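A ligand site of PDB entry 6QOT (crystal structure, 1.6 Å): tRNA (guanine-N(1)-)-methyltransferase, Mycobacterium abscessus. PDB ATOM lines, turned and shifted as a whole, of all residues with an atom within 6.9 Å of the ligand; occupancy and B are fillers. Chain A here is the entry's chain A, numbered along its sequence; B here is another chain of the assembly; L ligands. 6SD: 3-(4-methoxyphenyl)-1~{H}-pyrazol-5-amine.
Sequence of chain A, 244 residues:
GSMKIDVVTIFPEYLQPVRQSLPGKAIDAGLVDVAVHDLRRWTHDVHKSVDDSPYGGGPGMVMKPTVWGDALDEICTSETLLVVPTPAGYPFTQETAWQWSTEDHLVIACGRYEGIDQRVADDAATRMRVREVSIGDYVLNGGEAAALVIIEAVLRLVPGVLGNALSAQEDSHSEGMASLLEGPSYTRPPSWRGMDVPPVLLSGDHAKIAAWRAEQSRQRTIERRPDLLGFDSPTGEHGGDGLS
A nitrogen (N1) of the ligand lies within hydrogen-bond range of the backbone carbonyl oxygen (O) of Tyr 138. The backbone NH of Leu 140 is in hydrogen-bond range of a nitrogen (N2) of the ligand (2.9 Å). The side-chain hydroxyl (OG) of Ser 134 is in hydrogen-bond range of a nitrogen (N3) of the ligand, 3.1 Å away. A nitrogen (N3) of the ligand sits at hydrogen-bond distance from the backbone carbonyl oxygen (O) of Gly 136, 3.3 Å away.
The backbone carbonyl oxygen (O) of Gly 111 sits close to an oxygen (O) of the ligand (3.1 Å). A nitrogen (N3) of the ligand sits close to the backbone NH (N) of Ile 135, at 3.1 Å. Residues that only touch the ligand: Pro 85 (3.3 Å), Thr 86 (3.5 Å), Pro 87 (3.4 Å), Arg 112 (3.6 Å), Tyr 113 (3.2 Å), Gly 115 (3.8 Å), Val 139 (3.8 Å), Gly 142 (3.6 Å) and Gly 143 (3.4 Å). Hydrophobic or aromatic side chains that line the ligand: Pro 87, Ile 135 and Leu 140. Of the 29 residues printed, 15 come within 4 Å of the ligand. The nearest printed residue that does not touch the ligand is Asn 141 (4.01 Å).
The side-chain hydroxyl (OH) of Tyr 138 sits at hydrogen-bond distance from the backbone carbonyl oxygen (O) of Ile 135 (3.2 Å). The backbone carbonyl oxygen (O) of Gly 136 is in hydrogen-bond range of the side-chain hydroxyl (OG) of Ser 134 (3.0 Å). O of Val 133 sits at hydrogen-bond distance from N of Thr 86 (2.9 Å). OG1 of Thr 86 sits close to N of Ala 88. The side-chain carboxylate (OE2) of Glu 152 of chain B lies within hydrogen-bond range of the backbone NH (N) of Gly 142, 3.4 Å away. The guanidinium group (NE) of Arg 112 lies within salt-bridge range of the side-chain carboxylate (OE1) of Glu 144, at 2.9 Å. The backbone NH of Arg 112 lies within hydrogen-bond range of the side-chain sulfur of Met 63 (3.4 Å). The backbone carbonyl oxygen (O) of Gly 115 is in hydrogen-bond range of the backbone NH (N) of Met 63 (2.9 Å).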
ATOM      1  N   MET A  63      -8.362 -23.262   3.827  1.00  0.00           N
ATOM      2  CA  MET A  63      -9.017 -24.183   4.770  1.00  0.00           C
ATOM      3  C   MET A  63      -8.085 -25.351   5.157  1.00  0.00           C
ATOM      4  O   MET A  63      -7.356 -25.898   4.325  1.00  0.00           O
ATOM      5  CB  MET A  63     -10.342 -24.703   4.184  1.00  0.00           C
ATOM      6  CG  MET A  63     -11.367 -23.583   3.865  1.00  0.00           C
ATOM      7  SD  MET A  63     -13.054 -24.212   3.552  1.00  0.00           S
ATOM      8  CE  MET A  63     -13.875 -23.848   5.102  1.00  0.00           C
ATOM      9  N   VAL A  84     -15.902 -31.274  -5.827  1.00  0.00           N
ATOM     10  CA  VAL A  84     -15.338 -30.069  -5.209  1.00  0.00           C
ATOM     11  C   VAL A  84     -15.495 -28.846  -6.134  1.00  0.00           C
ATOM     12  O   VAL A  84     -14.723 -28.687  -7.098  1.00  0.00           O
ATOM     13  CB  VAL A  84     -13.843 -30.234  -4.867  1.00  0.00           C
ATOM     14  CG1 VAL A  84     -13.347 -29.047  -4.060  1.00  0.00           C
ATOM     15  CG2 VAL A  84     -13.597 -31.555  -4.107  1.00  0.00           C
ATOM     16  N   PRO A  85     -16.507 -27.995  -5.869  1.00  0.00           N
ATOM     17  CA  PRO A  85     -16.647 -26.798  -6.716  1.00  0.00           C
ATOM     18  C   PRO A  85     -15.485 -25.815  -6.538  1.00  0.00           C
ATOM     19  O   PRO A  85     -15.038 -25.600  -5.406  1.00  0.00           O
ATOM     20  CB  PRO A  85     -17.961 -26.176  -6.228  1.00  0.00           C
ATOM     21  CG  PRO A  85     -18.765 -27.340  -5.654  1.00  0.00           C
ATOM     22  CD  PRO A  85     -17.689 -28.212  -5.006  1.00  0.00           C
ATOM     23  N   THR A  86     -14.999 -25.245  -7.634  1.00  0.00           N
ATOM     24  CA  THR A  86     -13.860 -24.325  -7.584  1.00  0.00           C
ATOM     25  C   THR A  86     -13.787 -23.576  -8.922  1.00  0.00           C
ATOM     26  O   THR A  86     -14.080 -24.168  -9.955  1.00  0.00           O
ATOM     27  CB  THR A  86     -12.514 -25.063  -7.307  1.00  0.00           C
ATOM     28  OG1 THR A  86     -11.401 -24.203  -7.616  1.00  0.00           O
ATOM     29  CG2 THR A  86     -12.402 -26.369  -8.099  1.00  0.00           C
ATOM     30  N   PRO A  87     -13.403 -22.295  -8.903  1.00  0.00           N
ATOM     31  CA  PRO A  87     -13.261 -21.554 -10.178  1.00  0.00           C
ATOM     32  C   PRO A  87     -12.191 -22.159 -11.066  1.00  0.00           C
ATOM     33  O   PRO A  87     -12.227 -21.924 -12.283  1.00  0.00           O
ATOM     34  CB  PRO A  87     -12.847 -20.144  -9.736  1.00  0.00           C
ATOM     35  CG  PRO A  87     -13.152 -20.057  -8.283  1.00  0.00           C
ATOM     36  CD  PRO A  87     -13.079 -21.454  -7.736  1.00  0.00           C
ATOM     37  N   ALA A  88     -11.268 -22.927 -10.479  1.00  0.00           N
ATOM     38  CA  ALA A  88     -10.195 -23.561 -11.234  1.00  0.00           C
ATOM     39  C   ALA A  88     -10.534 -24.986 -11.710  1.00  0.00           C
ATOM     40  O   ALA A  88      -9.646 -25.735 -12.108  1.00  0.00           O
ATOM     41  CB  ALA A  88      -8.900 -23.569 -10.399  1.00  0.00           C
ATOM     42  N   GLY A  89     -11.816 -25.367 -11.670  1.00  0.00           N
ATOM     43  CA  GLY A  89     -12.183 -26.732 -12.007  1.00  0.00           C
ATOM     44  C   GLY A  89     -12.390 -27.010 -13.507  1.00  0.00           C
ATOM     45  O   GLY A  89     -12.408 -26.092 -14.325  1.00  0.00           O
ATOM     46  N   ALA A 109     -18.071 -31.076  -1.350  1.00  0.00           N
ATOM     47  CA  ALA A 109     -17.252 -30.342  -0.378  1.00  0.00           C
ATOM     48  C   ALA A 109     -17.237 -28.867  -0.732  1.00  0.00           C
ATOM     49  O   ALA A 109     -16.642 -28.489  -1.736  1.00  0.00           O
ATOM     50  CB  ALA A 109     -15.820 -30.876  -0.355  1.00  0.00           C
ATOM     51  N   CYS A 110     -17.890 -28.051   0.092  1.00  0.00           N
ATOM     52  CA  CYS A 110     -18.011 -26.612  -0.151  1.00  0.00           C
ATOM     53  C   CYS A 110     -16.902 -25.792   0.502  1.00  0.00           C
ATOM     54  O   CYS A 110     -16.808 -25.712   1.741  1.00  0.00           O
ATOM     55  CB  CYS A 110     -19.367 -26.101   0.344  1.00  0.00           C
ATOM     56  SG  CYS A 110     -20.804 -26.818  -0.505  1.00  0.00           S
ATOM     57  N   GLY A 111     -16.077 -25.134  -0.322  1.00  0.00           N
ATOM     58  CA  GLY A 111     -15.040 -24.270   0.209  1.00  0.00           C
ATOM     59  C   GLY A 111     -15.482 -22.857   0.529  1.00  0.00           C
ATOM     60  O   GLY A 111     -16.533 -22.378   0.033  1.00  0.00           O
ATOM     61  N   ARG A 112     -14.685 -22.180   1.363  1.00  0.00           N
ATOM     62  CA  ARG A 112     -14.813 -20.763   1.700  1.00  0.00           C
ATOM     63  C   ARG A 112     -13.386 -20.187   1.805  1.00  0.00           C
ATOM     64  O   ARG A 112     -12.416 -20.916   1.578  1.00  0.00           O
ATOM     65  CB  ARG A 112     -15.611 -20.548   3.000  1.00  0.00           C
ATOM     66  CG  ARG A 112     -17.124 -20.680   2.809  1.00  0.00           C
ATOM     67  CD  ARG A 112     -17.758 -19.351   2.403  1.00  0.00           C
ATOM     68  NE  ARG A 112     -19.038 -19.523   1.706  1.00  0.00           N
ATOM     69  CZ  ARG A 112     -19.844 -18.522   1.357  1.00  0.00           C
ATOM     70  NH1 ARG A 112     -19.516 -17.270   1.662  1.00  0.00           N
ATOM     71  NH2 ARG A 112     -20.977 -18.759   0.698  1.00  0.00           N
ATOM     72  N   TYR A 113     -13.251 -18.900   2.149  1.00  0.00           N
ATOM     73  CA  TYR A 113     -11.939 -18.243   2.132  1.00  0.00           C
ATOM     74  C   TYR A 113     -11.307 -18.395   0.746  1.00  0.00           C
ATOM     75  O   TYR A 113     -12.006 -18.274  -0.262  1.00  0.00           O
ATOM     76  CB  TYR A 113     -11.021 -18.814   3.228  1.00  0.00           C
ATOM     77  CG  TYR A 113     -11.618 -18.747   4.620  1.00  0.00           C
ATOM     78  CD1 TYR A 113     -12.367 -19.796   5.131  1.00  0.00           C
ATOM     79  CD2 TYR A 113     -11.435 -17.616   5.416  1.00  0.00           C
ATOM     80  CE1 TYR A 113     -12.922 -19.728   6.395  1.00  0.00           C
ATOM     81  CE2 TYR A 113     -11.978 -17.541   6.683  1.00  0.00           C
ATOM     82  CZ  TYR A 113     -12.722 -18.604   7.175  1.00  0.00           C
ATOM     83  OH  TYR A 113     -13.270 -18.546   8.432  1.00  0.00           O
ATOM     84  N   GLU A 114     -10.011 -18.702   0.652  1.00  0.00           N
ATOM     85  CA  GLU A 114      -9.358 -18.807  -0.661  1.00  0.00           C
ATOM     86  C   GLU A 114      -9.364 -20.220  -1.268  1.00  0.00           C
ATOM     87  O   GLU A 114      -8.906 -20.411  -2.392  1.00  0.00           O
ATOM     88  CB  GLU A 114      -7.928 -18.304  -0.575  1.00  0.00           C
ATOM     89  CG  GLU A 114      -7.833 -16.821  -0.219  1.00  0.00           C
ATOM     90  CD  GLU A 114      -8.657 -15.962  -1.161  1.00  0.00           C
ATOM     91  OE1 GLU A 114      -9.601 -15.292  -0.680  1.00  0.00           O
ATOM     92  OE2 GLU A 114      -8.369 -15.957  -2.374  1.00  0.00           O
ATOM     93  N   GLY A 115      -9.911 -21.199  -0.548  1.00  0.00           N
ATOM     94  CA  GLY A 115      -9.994 -22.562  -1.055  1.00  0.00           C
ATOM     95  C   GLY A 115      -9.513 -23.584  -0.046  1.00  0.00           C
ATOM     96  O   GLY A 115      -9.170 -23.208   1.068  1.00  0.00           O
ATOM     97  N   ILE A 116      -9.490 -24.867  -0.439  1.00  0.00           N
ATOM     98  CA  ILE A 116      -9.110 -25.964   0.483  1.00  0.00           C
ATOM     99  C   ILE A 116      -7.693 -26.424   0.179  1.00  0.00           C
ATOM    100  O   ILE A 116      -7.319 -26.545  -0.983  1.00  0.00           O
ATOM    101  CB  ILE A 116     -10.094 -27.175   0.362  1.00  0.00           C
ATOM    102  CG1 ILE A 116     -11.551 -26.704   0.524  1.00  0.00           C
ATOM    103  CG2 ILE A 116      -9.739 -28.303   1.371  1.00  0.00           C
ATOM    104  CD1 ILE A 116     -12.611 -27.749   0.154  1.00  0.00           C
ATOM    105  N   VAL A 133     -14.668 -29.108 -10.117  1.00  0.00           N
ATOM    106  CA  VAL A 133     -15.463 -28.572 -11.238  1.00  0.00           C
ATOM    107  C   VAL A 133     -15.875 -27.108 -11.063  1.00  0.00           C
ATOM    108  O   VAL A 133     -16.124 -26.655  -9.942  1.00  0.00           O
ATOM    109  CB  VAL A 133     -16.766 -29.393 -11.479  1.00  0.00           C
ATOM    110  CG1 VAL A 133     -16.440 -30.815 -11.929  1.00  0.00           C
ATOM    111  CG2 VAL A 133     -17.671 -29.394 -10.245  1.00  0.00           C
ATOM    112  N   SER A 134     -15.944 -26.403 -12.189  1.00  0.00           N
ATOM    113  CA  SER A 134     -16.456 -25.013 -12.228  1.00  0.00           C
ATOM    114  C   SER A 134     -17.841 -24.982 -12.871  1.00  0.00           C
ATOM    115  O   SER A 134     -18.080 -25.713 -13.837  1.00  0.00           O
ATOM    116  CB  SER A 134     -15.490 -24.112 -13.007  1.00  0.00           C
ATOM    117  OG  SER A 134     -16.070 -22.851 -13.304  1.00  0.00           O
ATOM    118  N   ILE A 135     -18.745 -24.147 -12.364  1.00  0.00           N
ATOM    119  CA  ILE A 135     -20.079 -24.031 -12.995  1.00  0.00           C
ATOM    120  C   ILE A 135     -20.223 -22.854 -13.970  1.00  0.00           C
ATOM    121  O   ILE A 135     -21.303 -22.653 -14.548  1.00  0.00           O
ATOM    122  CB  ILE A 135     -21.229 -23.944 -11.932  1.00  0.00           C
ATOM    123  CG1 ILE A 135     -21.088 -22.694 -11.030  1.00  0.00           C
ATOM    124  CG2 ILE A 135     -21.319 -25.242 -11.101  1.00  0.00           C
ATOM    125  CD1 ILE A 135     -22.437 -22.260 -10.384  1.00  0.00           C
ATOM    126  N   GLY A 136     -19.149 -22.078 -14.153  1.00  0.00           N
ATOM    127  CA  GLY A 136     -19.129 -20.974 -15.107  1.00  0.00           C
ATOM    128  C   GLY A 136     -17.960 -20.056 -14.863  1.00  0.00           C
ATOM    129  O   GLY A 136     -17.271 -20.180 -13.845  1.00  0.00           O
ATOM    130  N   ASP A 137     -17.734 -19.127 -15.786  1.00  0.00           N
ATOM    131  CA  ASP A 137     -16.553 -18.262 -15.724  1.00  0.00           C
ATOM    132  C   ASP A 137     -16.809 -16.974 -14.973  1.00  0.00           C
ATOM    133  O   ASP A 137     -16.742 -15.881 -15.540  1.00  0.00           O
ATOM    134  CB  ASP A 137     -16.056 -17.958 -17.128  1.00  0.00           C
ATOM    135  CG  ASP A 137     -15.486 -19.170 -17.822  1.00  0.00           C
ATOM    136  OD1 ASP A 137     -15.147 -20.151 -17.121  1.00  0.00           O
ATOM    137  OD2 ASP A 137     -15.372 -19.144 -19.063  1.00  0.00           O
ATOM    138  N   TYR A 138     -17.129 -17.132 -13.687  1.00  0.00           N
ATOM    139  CA  TYR A 138     -17.303 -16.035 -12.749  1.00  0.00           C
ATOM    140  C   TYR A 138     -16.839 -16.589 -11.407  1.00  0.00           C
ATOM    141  O   TYR A 138     -16.775 -17.812 -11.221  1.00  0.00           O
ATOM    142  CB  TYR A 138     -18.763 -15.559 -12.677  1.00  0.00           C
ATOM    143  CG  TYR A 138     -19.742 -16.713 -12.776  1.00  0.00           C
ATOM    144  CD1 TYR A 138     -19.993 -17.540 -11.687  1.00  0.00           C
ATOM    145  CD2 TYR A 138     -20.382 -17.007 -13.983  1.00  0.00           C
ATOM    146  CE1 TYR A 138     -20.851 -18.615 -11.779  1.00  0.00           C
ATOM    147  CE2 TYR A 138     -21.252 -18.084 -14.086  1.00  0.00           C
ATOM    148  CZ  TYR A 138     -21.487 -18.882 -12.993  1.00  0.00           C
ATOM    149  OH  TYR A 138     -22.341 -19.964 -13.054  1.00  0.00           O
ATOM    150  N   VAL A 139     -16.539 -15.691 -10.473  1.00  0.00           N
ATOM    151  CA  VAL A 139     -16.057 -16.096  -9.149  1.00  0.00           C
ATOM    152  C   VAL A 139     -17.108 -15.848  -8.065  1.00  0.00           C
ATOM    153  O   VAL A 139     -17.688 -14.765  -7.991  1.00  0.00           O
ATOM    154  CB  VAL A 139     -14.764 -15.321  -8.783  1.00  0.00           C
ATOM    155  CG1 VAL A 139     -14.270 -15.733  -7.371  1.00  0.00           C
ATOM    156  CG2 VAL A 139     -13.678 -15.583  -9.819  1.00  0.00           C
ATOM    157  N   LEU A 140     -17.351 -16.884  -7.238  1.00  0.00           N
ATOM    158  CA  LEU A 140     -18.268 -16.783  -6.094  1.00  0.00           C
ATOM    159  C   LEU A 140     -17.477 -16.622  -4.796  1.00  0.00           C
ATOM    160  O   LEU A 140     -16.255 -16.756  -4.799  1.00  0.00           O
ATOM    161  CB  LEU A 140     -19.166 -18.027  -6.016  1.00  0.00           C
ATOM    162  CG  LEU A 140     -19.978 -18.304  -7.288  1.00  0.00           C
ATOM    163  CD1 LEU A 140     -20.556 -19.700  -7.276  1.00  0.00           C
ATOM    164  CD2 LEU A 140     -21.107 -17.271  -7.423  1.00  0.00           C
ATOM    165  N   ASN A 141     -18.158 -16.359  -3.680  1.00  0.00           N
ATOM    166  CA  ASN A 141     -17.477 -16.294  -2.366  1.00  0.00           C
ATOM    167  C   ASN A 141     -17.132 -17.682  -1.811  1.00  0.00           C
ATOM    168  O   ASN A 141     -16.211 -17.827  -0.999  1.00  0.00           O
ATOM    169  CB  ASN A 141     -18.335 -15.572  -1.335  1.00  0.00           C
ATOM    170  CG  ASN A 141     -18.350 -14.067  -1.520  1.00  0.00           C
ATOM    171  OD1 ASN A 141     -17.372 -13.460  -1.961  1.00  0.00           O
ATOM    172  ND2 ASN A 141     -19.483 -13.454  -1.193  1.00  0.00           N
ATOM    173  N   GLY A 142     -17.909 -18.686  -2.211  1.00  0.00           N
ATOM    174  CA  GLY A 142     -17.710 -20.030  -1.719  1.00  0.00           C
ATOM    175  C   GLY A 142     -18.490 -21.017  -2.561  1.00  0.00           C
ATOM    176  O   GLY A 142     -19.183 -20.635  -3.486  1.00  0.00           O
ATOM    177  N   GLY A 143     -18.366 -22.300  -2.239  1.00  0.00           N
ATOM    178  CA  GLY A 143     -18.958 -23.337  -3.071  1.00  0.00           C
ATOM    179  C   GLY A 143     -20.459 -23.607  -2.925  1.00  0.00           C
ATOM    180  O   GLY A 143     -21.011 -24.385  -3.710  1.00  0.00           O
ATOM    181  N   GLU A 144     -21.096 -22.991  -1.928  1.00  0.00           N
ATOM    182  CA  GLU A 144     -22.499 -23.312  -1.619  1.00  0.00           C
ATOM    183  C   GLU A 144     -23.475 -23.069  -2.778  1.00  0.00           C
ATOM    184  O   GLU A 144     -24.304 -23.943  -3.089  1.00  0.00           O
ATOM    185  CB  GLU A 144     -22.971 -22.528  -0.378  1.00  0.00           C
ATOM    186  CG  GLU A 144     -22.371 -23.064   0.946  1.00  0.00           C
ATOM    187  CD  GLU A 144     -20.931 -22.600   1.217  1.00  0.00           C
ATOM    188  OE1 GLU A 144     -20.410 -21.733   0.479  1.00  0.00           O
ATOM    189  OE2 GLU A 144     -20.323 -23.115   2.171  1.00  0.00           O
ATOM    190  N   ALA A 146     -22.828 -22.990  -5.918  1.00  0.00           N
ATOM    191  CA  ALA A 146     -22.497 -23.970  -6.932  1.00  0.00           C
ATOM    192  C   ALA A 146     -23.073 -25.360  -6.580  1.00  0.00           C
ATOM    193  O   ALA A 146     -23.552 -26.071  -7.456  1.00  0.00           O
ATOM    194  CB  ALA A 146     -20.973 -24.046  -7.130  1.00  0.00           C
ATOM    195  N   GLU B 152     -24.695 -13.303  -5.839  1.00  0.00           N
ATOM    196  CA  GLU B 152     -23.420 -13.492  -5.156  1.00  0.00           C
ATOM    197  C   GLU B 152     -22.244 -12.941  -5.974  1.00  0.00           C
ATOM    198  O   GLU B 152     -21.383 -12.237  -5.427  1.00  0.00           O
ATOM    199  CB  GLU B 152     -23.196 -14.975  -4.850  1.00  0.00           C
ATOM    200  CG  GLU B 152     -21.846 -15.259  -4.226  1.00  0.00           C
ATOM    201  CD  GLU B 152     -21.855 -16.503  -3.343  1.00  0.00           C
ATOM    202  OE1 GLU B 152     -22.954 -16.963  -2.950  1.00  0.00           O
ATOM    203  OE2 GLU B 152     -20.761 -17.014  -3.063  1.00  0.00           O
HETATM  204  C1  6SD L   1     -13.509 -20.684  -1.798  1.00  0.00           C
HETATM  205  C2  6SD L   1     -15.000 -21.453  -3.522  1.00  0.00           C
HETATM  206  C3  6SD L   1     -15.558 -22.541  -4.199  1.00  0.00           C
HETATM  207  C7  6SD L   1     -14.963 -20.196  -4.109  1.00  0.00           C
HETATM  208  C8  6SD L   1     -16.586 -20.861  -7.495  1.00  0.00           C
HETATM  209  C9  6SD L   1     -16.812 -21.809  -8.484  1.00  0.00           C
HETATM  210  C10 6SD L   1     -17.203 -21.112  -9.616  1.00  0.00           C
HETATM  211  N3  6SD L   1     -17.545 -21.665 -10.879  1.00  0.00           N
HETATM  212  N1  6SD L   1     -17.182 -19.789  -9.317  1.00  0.00           N
HETATM  213  N2  6SD L   1     -16.790 -19.661  -8.025  1.00  0.00           N
HETATM  214  C5  6SD L   1     -16.073 -21.095  -6.071  1.00  0.00           C
HETATM  215  C4  6SD L   1     -16.093 -22.369  -5.484  1.00  0.00           C
HETATM  216  C6  6SD L   1     -15.488 -20.026  -5.395  1.00  0.00           C
HETATM  217  O   6SD L   1     -14.467 -21.643  -2.225  1.00  0.00           O
